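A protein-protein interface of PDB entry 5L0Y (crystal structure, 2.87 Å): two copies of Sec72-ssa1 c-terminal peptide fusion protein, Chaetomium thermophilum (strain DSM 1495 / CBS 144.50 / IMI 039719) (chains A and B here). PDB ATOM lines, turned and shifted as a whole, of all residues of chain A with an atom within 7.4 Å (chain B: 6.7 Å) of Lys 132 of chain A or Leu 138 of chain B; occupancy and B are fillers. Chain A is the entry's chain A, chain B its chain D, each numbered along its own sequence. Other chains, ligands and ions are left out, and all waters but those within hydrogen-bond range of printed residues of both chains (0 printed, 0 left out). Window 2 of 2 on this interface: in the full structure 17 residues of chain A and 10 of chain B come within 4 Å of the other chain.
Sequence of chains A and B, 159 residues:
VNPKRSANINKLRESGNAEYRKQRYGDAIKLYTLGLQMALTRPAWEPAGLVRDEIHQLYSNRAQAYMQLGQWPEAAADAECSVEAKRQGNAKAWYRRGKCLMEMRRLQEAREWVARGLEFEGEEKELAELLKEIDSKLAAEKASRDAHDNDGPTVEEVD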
ATOM      1  N   ARG A 111       0.946  14.938 -29.948  1.00  0.00           N
ATOM      2  CA  ARG A 111       1.297  14.763 -28.545  1.00  0.00           C
ATOM      3  C   ARG A 111       2.666  15.367 -28.263  1.00  0.00           C
ATOM      4  O   ARG A 111       2.810  16.205 -27.372  1.00  0.00           O
ATOM      5  CB  ARG A 111       1.269  13.276 -28.176  1.00  0.00           C
ATOM      6  CG  ARG A 111       2.173  12.885 -27.015  1.00  0.00           C
ATOM      7  CD  ARG A 111       1.540  13.146 -25.658  1.00  0.00           C
ATOM      8  NE  ARG A 111       2.508  12.940 -24.582  1.00  0.00           N
ATOM      9  CZ  ARG A 111       2.238  13.065 -23.287  1.00  0.00           C
ATOM     10  NH1 ARG A 111       1.020  13.390 -22.886  1.00  0.00           N
ATOM     11  NH2 ARG A 111       3.189  12.862 -22.388  1.00  0.00           N
ATOM     12  N   VAL A 114       2.550  19.175 -28.864  1.00  0.00           N
ATOM     13  CA  VAL A 114       1.940  19.910 -27.791  1.00  0.00           C
ATOM     14  C   VAL A 114       2.816  19.934 -26.568  1.00  0.00           C
ATOM     15  O   VAL A 114       2.939  20.948 -25.961  1.00  0.00           O
ATOM     16  CB  VAL A 114       0.535  19.421 -27.487  1.00  0.00           C
ATOM     17  CG1 VAL A 114      -0.010  20.119 -26.281  1.00  0.00           C
ATOM     18  CG2 VAL A 114      -0.363  19.719 -28.652  1.00  0.00           C
ATOM     19  N   LEU A 118       4.530  23.075 -24.918  1.00  0.00           N
ATOM     20  CA  LEU A 118       4.276  23.453 -23.563  1.00  0.00           C
ATOM     21  C   LEU A 118       5.530  23.895 -22.958  1.00  0.00           C
ATOM     22  O   LEU A 118       5.578  25.064 -22.627  1.00  0.00           O
ATOM     23  CB  LEU A 118       3.785  22.278 -22.760  1.00  0.00           C
ATOM     24  CG  LEU A 118       2.282  22.252 -22.686  1.00  0.00           C
ATOM     25  CD1 LEU A 118       1.787  21.061 -21.930  1.00  0.00           C
ATOM     26  CD2 LEU A 118       1.786  23.508 -22.045  1.00  0.00           C
ATOM     27  N   GLU A 126      -4.336  26.166 -21.969  1.00  0.00           N
ATOM     28  CA  GLU A 126      -5.071  25.703 -23.157  1.00  0.00           C
ATOM     29  C   GLU A 126      -4.351  24.605 -23.933  1.00  0.00           C
ATOM     30  O   GLU A 126      -4.954  23.586 -24.316  1.00  0.00           O
ATOM     31  CB  GLU A 126      -5.367  26.867 -24.089  1.00  0.00           C
ATOM     32  CG  GLU A 126      -6.774  26.814 -24.646  1.00  0.00           C
ATOM     33  CD  GLU A 126      -7.577  28.040 -24.279  1.00  0.00           C
ATOM     34  OE1 GLU A 126      -7.273  29.127 -24.811  1.00  0.00           O
ATOM     35  OE2 GLU A 126      -8.511  27.927 -23.455  1.00  0.00           O
ATOM     36  N   LEU A 127      -3.060  24.825 -24.149  1.00  0.00           N
ATOM     37  CA  LEU A 127      -2.187  23.779 -24.628  1.00  0.00           C
ATOM     38  C   LEU A 127      -2.403  22.515 -23.809  1.00  0.00           C
ATOM     39  O   LEU A 127      -2.667  21.454 -24.365  1.00  0.00           O
ATOM     40  CB  LEU A 127      -0.728  24.214 -24.553  1.00  0.00           C
ATOM     41  CG  LEU A 127      -0.223  25.105 -25.682  1.00  0.00           C
ATOM     42  CD1 LEU A 127       1.280  25.312 -25.570  1.00  0.00           C
ATOM     43  CD2 LEU A 127      -0.576  24.481 -27.014  1.00  0.00           C
ATOM     44  N   ALA A 128      -2.323  22.637 -22.487  1.00  0.00           N
ATOM     45  CA  ALA A 128      -2.398  21.460 -21.628  1.00  0.00           C
ATOM     46  C   ALA A 128      -3.743  20.758 -21.746  1.00  0.00           C
ATOM     47  O   ALA A 128      -3.783  19.534 -21.789  1.00  0.00           O
ATOM     48  CB  ALA A 128      -2.125  21.831 -20.178  1.00  0.00           C
ATOM     49  N   GLU A 129      -4.838  21.515 -21.797  1.00  0.00           N
ATOM     50  CA  GLU A 129      -6.154  20.899 -21.957  1.00  0.00           C
ATOM     51  C   GLU A 129      -6.169  20.066 -23.232  1.00  0.00           C
ATOM     52  O   GLU A 129      -6.605  18.898 -23.227  1.00  0.00           O
ATOM     53  CB  GLU A 129      -7.266  21.950 -21.987  1.00  0.00           C
ATOM     54  CG  GLU A 129      -7.833  22.301 -20.621  1.00  0.00           C
ATOM     55  CD  GLU A 129      -9.073  23.178 -20.705  1.00  0.00           C
ATOM     56  OE1 GLU A 129      -9.779  23.118 -21.733  1.00  0.00           O
ATOM     57  OE2 GLU A 129      -9.345  23.923 -19.738  1.00  0.00           O
ATOM     58  N   LEU A 130      -5.670  20.662 -24.317  1.00  0.00           N
ATOM     59  CA  LEU A 130      -5.552  19.935 -25.582  1.00  0.00           C
ATOM     60  C   LEU A 130      -4.702  18.666 -25.438  1.00  0.00           C
ATOM     61  O   LEU A 130      -5.037  17.625 -25.993  1.00  0.00           O
ATOM     62  CB  LEU A 130      -4.962  20.832 -26.675  1.00  0.00           C
ATOM     63  CG  LEU A 130      -4.789  20.199 -28.061  1.00  0.00           C
ATOM     64  CD1 LEU A 130      -6.131  19.772 -28.624  1.00  0.00           C
ATOM     65  CD2 LEU A 130      -4.107  21.156 -29.013  1.00  0.00           C
ATOM     66  N   LEU A 131      -3.603  18.757 -24.697  1.00  0.00           N
ATOM     67  CA  LEU A 131      -2.720  17.611 -24.483  1.00  0.00           C
ATOM     68  C   LEU A 131      -3.449  16.473 -23.783  1.00  0.00           C
ATOM     69  O   LEU A 131      -3.381  15.314 -24.208  1.00  0.00           O
ATOM     70  CB  LEU A 131      -1.496  18.028 -23.663  1.00  0.00           C
ATOM     71  CG  LEU A 131      -0.563  16.913 -23.188  1.00  0.00           C
ATOM     72  CD1 LEU A 131      -0.134  16.058 -24.363  1.00  0.00           C
ATOM     73  CD2 LEU A 131       0.656  17.463 -22.445  1.00  0.00           C
ATOM     74  N   LYS A 132      -4.131  16.821 -22.698  1.00  0.00           N
ATOM     75  CA  LYS A 132      -4.940  15.872 -21.963  1.00  0.00           C
ATOM     76  C   LYS A 132      -5.900  15.163 -22.918  1.00  0.00           C
ATOM     77  O   LYS A 132      -5.982  13.926 -22.925  1.00  0.00           O
ATOM     78  CB  LYS A 132      -5.694  16.583 -20.843  1.00  0.00           C
ATOM     79  CG  LYS A 132      -5.444  16.031 -19.453  1.00  0.00           C
ATOM     80  CD  LYS A 132      -6.505  15.025 -19.081  1.00  0.00           C
ATOM     81  CE  LYS A 132      -6.216  13.650 -19.640  1.00  0.00           C
ATOM     82  NZ  LYS A 132      -7.437  13.150 -20.318  1.00  0.00           N
ATOM     83  N   GLU A 133      -6.591  15.951 -23.743  1.00  0.00           N
ATOM     84  CA  GLU A 133      -7.413  15.389 -24.812  1.00  0.00           C
ATOM     85  C   GLU A 133      -6.653  14.374 -25.684  1.00  0.00           C
ATOM     86  O   GLU A 133      -7.155  13.266 -25.944  1.00  0.00           O
ATOM     87  CB  GLU A 133      -7.964  16.507 -25.686  1.00  0.00           C
ATOM     88  CG  GLU A 133      -9.452  16.412 -25.983  1.00  0.00           C
ATOM     89  CD  GLU A 133      -9.993  17.680 -26.618  1.00  0.00           C
ATOM     90  OE1 GLU A 133     -10.715  18.426 -25.920  1.00  0.00           O
ATOM     91  OE2 GLU A 133      -9.695  17.930 -27.806  1.00  0.00           O
ATOM     92  N   ILE A 134      -5.456  14.751 -26.132  1.00  0.00           N
ATOM     93  CA  ILE A 134      -4.643  13.879 -26.972  1.00  0.00           C
ATOM     94  C   ILE A 134      -4.381  12.537 -26.289  1.00  0.00           C
ATOM     95  O   ILE A 134      -4.567  11.477 -26.895  1.00  0.00           O
ATOM     96  CB  ILE A 134      -3.283  14.534 -27.345  1.00  0.00           C
ATOM     97  CG1 ILE A 134      -3.487  15.863 -28.076  1.00  0.00           C
ATOM     98  CG2 ILE A 134      -2.448  13.589 -28.192  1.00  0.00           C
ATOM     99  CD1 ILE A 134      -2.190  16.501 -28.580  1.00  0.00           C
ATOM    100  N   ASP A 135      -3.967  12.585 -25.024  1.00  0.00           N
ATOM    101  CA  ASP A 135      -3.693  11.368 -24.264  1.00  0.00           C
ATOM    102  C   ASP A 135      -4.933  10.485 -24.096  1.00  0.00           C
ATOM    103  O   ASP A 135      -4.858   9.270 -24.291  1.00  0.00           O
ATOM    104  CB  ASP A 135      -3.113  11.716 -22.893  1.00  0.00           C
ATOM    105  CG  ASP A 135      -1.682  12.207 -22.975  1.00  0.00           C
ATOM    106  OD1 ASP A 135      -1.005  11.897 -23.979  1.00  0.00           O
ATOM    107  OD2 ASP A 135      -1.234  12.889 -22.024  1.00  0.00           O
ATOM    108  N   SER A 136      -6.065  11.086 -23.736  1.00  0.00           N
ATOM    109  CA  SER A 136      -7.310  10.325 -23.657  1.00  0.00           C
ATOM    110  C   SER A 136      -7.618   9.604 -24.955  1.00  0.00           C
ATOM    111  O   SER A 136      -7.949   8.408 -24.947  1.00  0.00           O
ATOM    112  CB  SER A 136      -8.484  11.232 -23.310  1.00  0.00           C
ATOM    113  OG  SER A 136      -8.018  12.442 -22.758  1.00  0.00           O
ATOM    114  N   LYS A 137      -7.518  10.339 -26.063  1.00  0.00           N
ATOM    115  CA  LYS A 137      -7.784   9.778 -27.390  1.00  0.00           C
ATOM    116  C   LYS A 137      -6.831   8.637 -27.760  1.00  0.00           C
ATOM    117  O   LYS A 137      -7.248   7.621 -28.321  1.00  0.00           O
ATOM    118  CB  LYS A 137      -7.700  10.879 -28.443  1.00  0.00           C
ATOM    119  CG  LYS A 137      -8.455  10.611 -29.728  1.00  0.00           C
ATOM    120  CD  LYS A 137      -8.504  11.874 -30.574  1.00  0.00           C
ATOM    121  CE  LYS A 137      -9.239  13.003 -29.852  1.00  0.00           C
ATOM    122  NZ  LYS A 137     -10.671  12.662 -29.613  1.00  0.00           N
ATOM    123  N   LEU A 138      -5.552   8.824 -27.451  1.00  0.00           N
ATOM    124  CA  LEU A 138      -4.536   7.790 -27.636  1.00  0.00           C
ATOM    125  C   LEU A 138      -4.899   6.518 -26.893  1.00  0.00           C
ATOM    126  O   LEU A 138      -5.026   5.450 -27.495  1.00  0.00           O
ATOM    127  CB  LEU A 138      -3.170   8.284 -27.159  1.00  0.00           C
ATOM    128  CG  LEU A 138      -2.386   9.188 -28.106  1.00  0.00           C
ATOM    129  CD1 LEU A 138      -1.203   9.828 -27.389  1.00  0.00           C
ATOM    130  CD2 LEU A 138      -1.914   8.380 -29.298  1.00  0.00           C
ATOM    131  N   LEU B 107      -6.796  13.864  -9.117  1.00  0.00           N
ATOM    132  CA  LEU B 107      -7.022  13.145 -10.365  1.00  0.00           C
ATOM    133  C   LEU B 107      -5.859  13.215 -11.352  1.00  0.00           C
ATOM    134  O   LEU B 107      -5.493  12.207 -11.951  1.00  0.00           O
ATOM    135  CB  LEU B 107      -8.288  13.672 -11.039  1.00  0.00           C
ATOM    136  CG  LEU B 107      -9.558  13.785 -10.193  1.00  0.00           C
ATOM    137  CD1 LEU B 107      -9.661  15.148  -9.510  1.00  0.00           C
ATOM    138  CD2 LEU B 107     -10.778  13.513 -11.053  1.00  0.00           C
ATOM    139  N   GLN B 108      -5.297  14.405 -11.533  1.00  0.00           N
ATOM    140  CA  GLN B 108      -4.192  14.601 -12.471  1.00  0.00           C
ATOM    141  C   GLN B 108      -3.001  13.700 -12.129  1.00  0.00           C
ATOM    142  O   GLN B 108      -2.458  12.993 -12.991  1.00  0.00           O
ATOM    143  CB  GLN B 108      -3.761  16.071 -12.477  1.00  0.00           C
ATOM    144  CG  GLN B 108      -4.896  17.051 -12.748  1.00  0.00           C
ATOM    145  CD  GLN B 108      -4.514  18.492 -12.454  1.00  0.00           C
ATOM    146  OE1 GLN B 108      -3.486  18.760 -11.834  1.00  0.00           O
ATOM    147  NE2 GLN B 108      -5.346  19.426 -12.901  1.00  0.00           N
ATOM    148  N   ARG B 111      -3.659  10.145 -12.824  1.00  0.00           N
ATOM    149  CA  ARG B 111      -3.496   9.925 -14.259  1.00  0.00           C
ATOM    150  C   ARG B 111      -2.038   9.663 -14.601  1.00  0.00           C
ATOM    151  O   ARG B 111      -1.701   8.653 -15.236  1.00  0.00           O
ATOM    152  CB  ARG B 111      -4.016  11.139 -15.042  1.00  0.00           C
ATOM    153  CG  ARG B 111      -3.655  11.159 -16.526  1.00  0.00           C
ATOM    154  CD  ARG B 111      -4.535  10.208 -17.310  1.00  0.00           C
ATOM    155  NE  ARG B 111      -4.170  10.132 -18.723  1.00  0.00           N
ATOM    156  CZ  ARG B 111      -4.770   9.332 -19.601  1.00  0.00           C
ATOM    157  NH1 ARG B 111      -5.763   8.542 -19.215  1.00  0.00           N
ATOM    158  NH2 ARG B 111      -4.380   9.319 -20.867  1.00  0.00           N
ATOM    159  N   GLU B 133     -11.183   5.329 -16.607  1.00  0.00           N
ATOM    160  CA  GLU B 133     -12.102   5.919 -15.649  1.00  0.00           C
ATOM    161  C   GLU B 133     -11.580   7.264 -15.142  1.00  0.00           C
ATOM    162  O   GLU B 133     -12.358   8.215 -14.962  1.00  0.00           O
ATOM    163  CB  GLU B 133     -12.338   4.962 -14.479  1.00  0.00           C
ATOM    164  CG  GLU B 133     -13.480   5.376 -13.559  1.00  0.00           C
ATOM    165  CD  GLU B 133     -13.500   4.612 -12.241  1.00  0.00           C
ATOM    166  OE1 GLU B 133     -12.822   3.566 -12.136  1.00  0.00           O
ATOM    167  OE2 GLU B 133     -14.195   5.067 -11.307  1.00  0.00           O
ATOM    168  N   ILE B 134     -10.267   7.347 -14.929  1.00  0.00           N
ATOM    169  CA  ILE B 134      -9.650   8.587 -14.456  1.00  0.00           C
ATOM    170  C   ILE B 134      -9.798   9.741 -15.466  1.00  0.00           C
ATOM    171  O   ILE B 134     -10.298  10.818 -15.102  1.00  0.00           O
ATOM    172  CB  ILE B 134      -8.148   8.382 -14.111  1.00  0.00           C
ATOM    173  CG1 ILE B 134      -8.003   7.434 -12.922  1.00  0.00           C
ATOM    174  CG2 ILE B 134      -7.472   9.715 -13.804  1.00  0.00           C
ATOM    175  CD1 ILE B 134      -6.579   7.257 -12.445  1.00  0.00           C
ATOM    176  N   ASP B 135      -9.399   9.544 -16.726  1.00  0.00           N
ATOM    177  CA  ASP B 135      -9.504  10.674 -17.652  1.00  0.00           C
ATOM    178  C   ASP B 135     -10.975  10.914 -18.059  1.00  0.00           C
ATOM    179  O   ASP B 135     -11.318  12.000 -18.545  1.00  0.00           O
ATOM    180  CB  ASP B 135      -8.588  10.497 -18.887  1.00  0.00           C
ATOM    181  CG  ASP B 135      -8.851   9.217 -19.663  1.00  0.00           C
ATOM    182  OD1 ASP B 135     -10.014   8.766 -19.741  1.00  0.00           O
ATOM    183  OD2 ASP B 135      -7.881   8.660 -20.235  1.00  0.00           O
ATOM    184  N   SER B 136     -11.842   9.924 -17.823  1.00  0.00           N
ATOM    185  CA  SER B 136     -13.290  10.122 -17.992  1.00  0.00           C
ATOM    186  C   SER B 136     -13.827  11.127 -16.963  1.00  0.00           C
ATOM    187  O   SER B 136     -14.488  12.130 -17.310  1.00  0.00           O
ATOM    188  CB  SER B 136     -14.034   8.788 -17.878  1.00  0.00           C
ATOM    189  OG  SER B 136     -15.422   8.995 -17.711  1.00  0.00           O
ATOM    190  N   LYS B 137     -13.541  10.839 -15.695  1.00  0.00           N
ATOM    191  CA  LYS B 137     -13.811  11.791 -14.622  1.00  0.00           C
ATOM    192  C   LYS B 137     -13.252  13.190 -14.953  1.00  0.00           C
ATOM    193  O   LYS B 137     -13.969  14.203 -14.846  1.00  0.00           O
ATOM    194  CB  LYS B 137     -13.225  11.286 -13.300  1.00  0.00           C
ATOM    195  CG  LYS B 137     -14.086  10.246 -12.561  1.00  0.00           C
ATOM    196  CD  LYS B 137     -13.672  10.135 -11.084  1.00  0.00           C
ATOM    197  CE  LYS B 137     -14.725   9.437 -10.209  1.00  0.00           C
ATOM    198  NZ  LYS B 137     -14.704   7.950 -10.326  1.00  0.00           N
ATOM    199  N   LEU B 138     -11.982  13.238 -15.359  1.00  0.00           N
ATOM    200  CA  LEU B 138     -11.363  14.493 -15.802  1.00  0.00           C
ATOM    201  C   LEU B 138     -12.209  15.253 -16.828  1.00  0.00           C
ATOM    202  O   LEU B 138     -12.425  16.468 -16.694  1.00  0.00           O
ATOM    203  CB  LEU B 138      -9.968  14.228 -16.374  1.00  0.00           C
ATOM    204  CG  LEU B 138      -8.877  14.043 -15.316  1.00  0.00           C
ATOM    205  CD1 LEU B 138      -7.483  14.223 -15.897  1.00  0.00           C
ATOM    206  CD2 LEU B 138      -9.118  15.011 -14.169  1.00  0.00           C
ATOM    207  N   ALA B 139     -12.680  14.539 -17.850  1.00  0.00           N
ATOM    208  CA  ALA B 139     -13.618  15.124 -18.810  1.00  0.00           C
ATOM    209  C   ALA B 139     -14.819  15.765 -18.118  1.00  0.00           C
ATOM    210  O   ALA B 139     -15.173  16.933 -18.401  1.00  0.00           O
ATOM    211  CB  ALA B 139     -14.089  14.075 -19.785  1.00  0.00           C
ATOM    212  N   ALA B 140     -15.444  14.996 -17.222  1.00  0.00           N
ATOM    213  CA  ALA B 140     -16.556  15.511 -16.422  1.00  0.00           C
ATOM    214  C   ALA B 140     -16.232  16.863 -15.769  1.00  0.00           C
ATOM    215  O   ALA B 140     -17.044  17.786 -15.831  1.00  0.00           O
ATOM    216  CB  ALA B 140     -16.961  14.498 -15.362  1.00  0.00           C
ATOM    217  N   GLU B 141     -15.059  16.991 -15.151  1.00  0.00           N
ATOM    218  CA  GLU B 141     -14.693  18.293 -14.577  1.00  0.00           C
ATOM    219  C   GLU B 141     -14.548  19.389 -15.632  1.00  0.00           C
ATOM    220  O   GLU B 141     -15.100  20.490 -15.476  1.00  0.00           O
ATOM    221  CB  GLU B 141     -13.395  18.190 -13.775  1.00  0.00           C
ATOM    222  CG  GLU B 141     -13.564  17.601 -12.399  1.00  0.00           C
ATOM    223  CD  GLU B 141     -12.591  16.479 -12.143  1.00  0.00           C
ATOM    224  OE1 GLU B 141     -12.628  15.484 -12.892  1.00  0.00           O
ATOM    225  OE2 GLU B 141     -11.776  16.597 -11.208  1.00  0.00           O
ATOM    226  N   LYS B 142     -13.808  19.094 -16.698  1.00  0.00           N
ATOM    227  CA  LYS B 142     -13.533  20.116 -17.708  1.00  0.00           C
ATOM    228  C   LYS B 142     -14.812  20.750 -18.261  1.00  0.00           C
ATOM    229  O   LYS B 142     -14.925  21.994 -18.394  1.00  0.00           O
ATOM    230  CB  LYS B 142     -12.713  19.533 -18.851  1.00  0.00           C
ATOM    231  CG  LYS B 142     -12.014  20.611 -19.651  1.00  0.00           C
ATOM    232  CD  LYS B 142     -11.316  21.599 -18.710  1.00  0.00           C
ATOM    233  CE  LYS B 142     -10.042  21.012 -18.092  1.00  0.00           C
ATOM    234  NZ  LYS B 142      -9.694  21.628 -16.771  1.00  0.00           N
ATOM    235  N   ALA B 143     -15.777  19.884 -18.559  1.00  0.00           N
ATOM    236  CA  ALA B 143     -17.091  20.339 -18.983  1.00  0.00           C
ATOM    237  C   ALA B 143     -17.685  21.398 -18.037  1.00  0.00           C
ATOM    238  O   ALA B 143     -18.015  22.505 -18.471  1.00  0.00           O
ATOM    239  CB  ALA B 143     -18.020  19.156 -19.104  1.00  0.00           C
ATOM    240  N   ARG B 145     -16.269  23.206 -15.788  1.00  0.00           N
ATOM    241  CA  ARG B 145     -15.461  24.425 -15.789  1.00  0.00           C
ATOM    242  C   ARG B 145     -15.822  25.333 -16.954  1.00  0.00           C
ATOM    243  O   ARG B 145     -15.819  26.568 -16.814  1.00  0.00           O
ATOM    244  CB  ARG B 145     -13.971  24.094 -15.839  1.00  0.00           C
ATOM    245  CG  ARG B 145     -13.534  23.119 -14.772  1.00  0.00           C
ATOM    246  CD  ARG B 145     -12.049  22.836 -14.816  1.00  0.00           C
ATOM    247  NE  ARG B 145     -11.419  23.403 -13.632  1.00  0.00           N
ATOM    248  CZ  ARG B 145     -11.510  22.877 -12.416  1.00  0.00           C
ATOM    249  NH1 ARG B 145     -10.920  23.476 -11.396  1.00  0.00           N
ATOM    250  NH2 ARG B 145     -12.187  21.754 -12.224  1.00  0.00           N
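The side-chain amino group (NZ) of Lys 142 of chain B lies within salt-bridge range of the side-chain carboxylate (OE2) of Glu 129 of chain A (3.8 Å). The backbone carbonyl oxygen (O) of Asp 135 of chain A lies close to the guanidinium group (NH2) of Arg 111 of chain B (3.5 Å).
The guanidinium group (NH1) of Arg 111 of chain A is in salt-bridge range of the side-chain carboxylate (OD2) of Asp 135 of chain A (2.5 Å). The backbone carbonyl oxygen of Lys 132 of chain A sits at hydrogen-bond distance from the side-chain hydroxyl of Ser 136 of chain A (2.5 Å). The side-chain hydroxyl of Ser 136 of chain A sits at hydrogen-bond distance from the backbone carbonyl oxygen of Glu 133 of chain A, at 3.4 Å. OD2 of Asp 135 of chain B lies within salt-bridge range of NH2 of Arg 111 of chain B (3.6 Å). The side-chain carboxylate (OE1) of Glu 141 of chain B sits close to the backbone NH (N) of Leu 138 of chain B, 3.4 Å away.
Among the printed residues, pairs that only touch across the chains: Lys 132 of chain A with Asp 135 of chain B (3.2 Å), Lys 132 of chain A with Leu 138 of chain B (3.4 Å), Ser 136 of chain A with Arg 111 of chain B (3.8 Å) and Ser 136 of chain A with Asp 135 of chain B (3.8 Å).
Of chain B, only Asp 135 and Leu 138 come within 4 Å of Lys 132 of chain A. Of chain A, only Lys 132 (3.4 Å) comes within 4 Å of Leu 138 of chain B. Printed residues of chain B within 4 Å of Asp 135 of chain A: Arg 111 (3.4 Å). Printed residues of chain A within 4 Å of Lys 142 of chain B: Glu 129. Of the printed residues of chain B, Ser 136 of chain A touches Arg 111 and Asp 135. The nearest residue of chain B that does not touch Lys 132 of chain A is Arg 111 of chain B (4.2 Å).
Of the 15 printed residues of chain B, 4 touch a printed residue of chain A. Hydrophobic or aromatic side chains of chain B that line the printed part of chain A: Leu 138. Of the 16 printed residues of chain A, 4 touch a printed residue of chain B. Along chain A the printed residues that touch a printed residue of chain B span positions 129 to 136. Among the printed residues, Asp or Glu carboxylates within 4 Å of a Lys or Arg side-chain nitrogen of the other chain: Glu 129 of chain A with Lys 142 of chain B (3.8 Å).
Asp 135 of chain A touches Arg 111 of chain B, but with the chains exchanged Arg 111 of chain A does not touch Asp 135 of chain B (10.4 Å). Ser 136 of chain A touches Arg 111 of chain B, but with the chains exchanged Arg 111 of chain A does not touch Ser 136 of chain B (14.3 Å). Ser 136 of chain A touches Asp 135 of chain B, but with the chains exchanged Asp 135 of chain A does not touch Ser 136 of chain B (9.3 Å). Of the 6 pairs that touch across the chains among the printed residues, none has its exchanged pair printed and touching as well.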
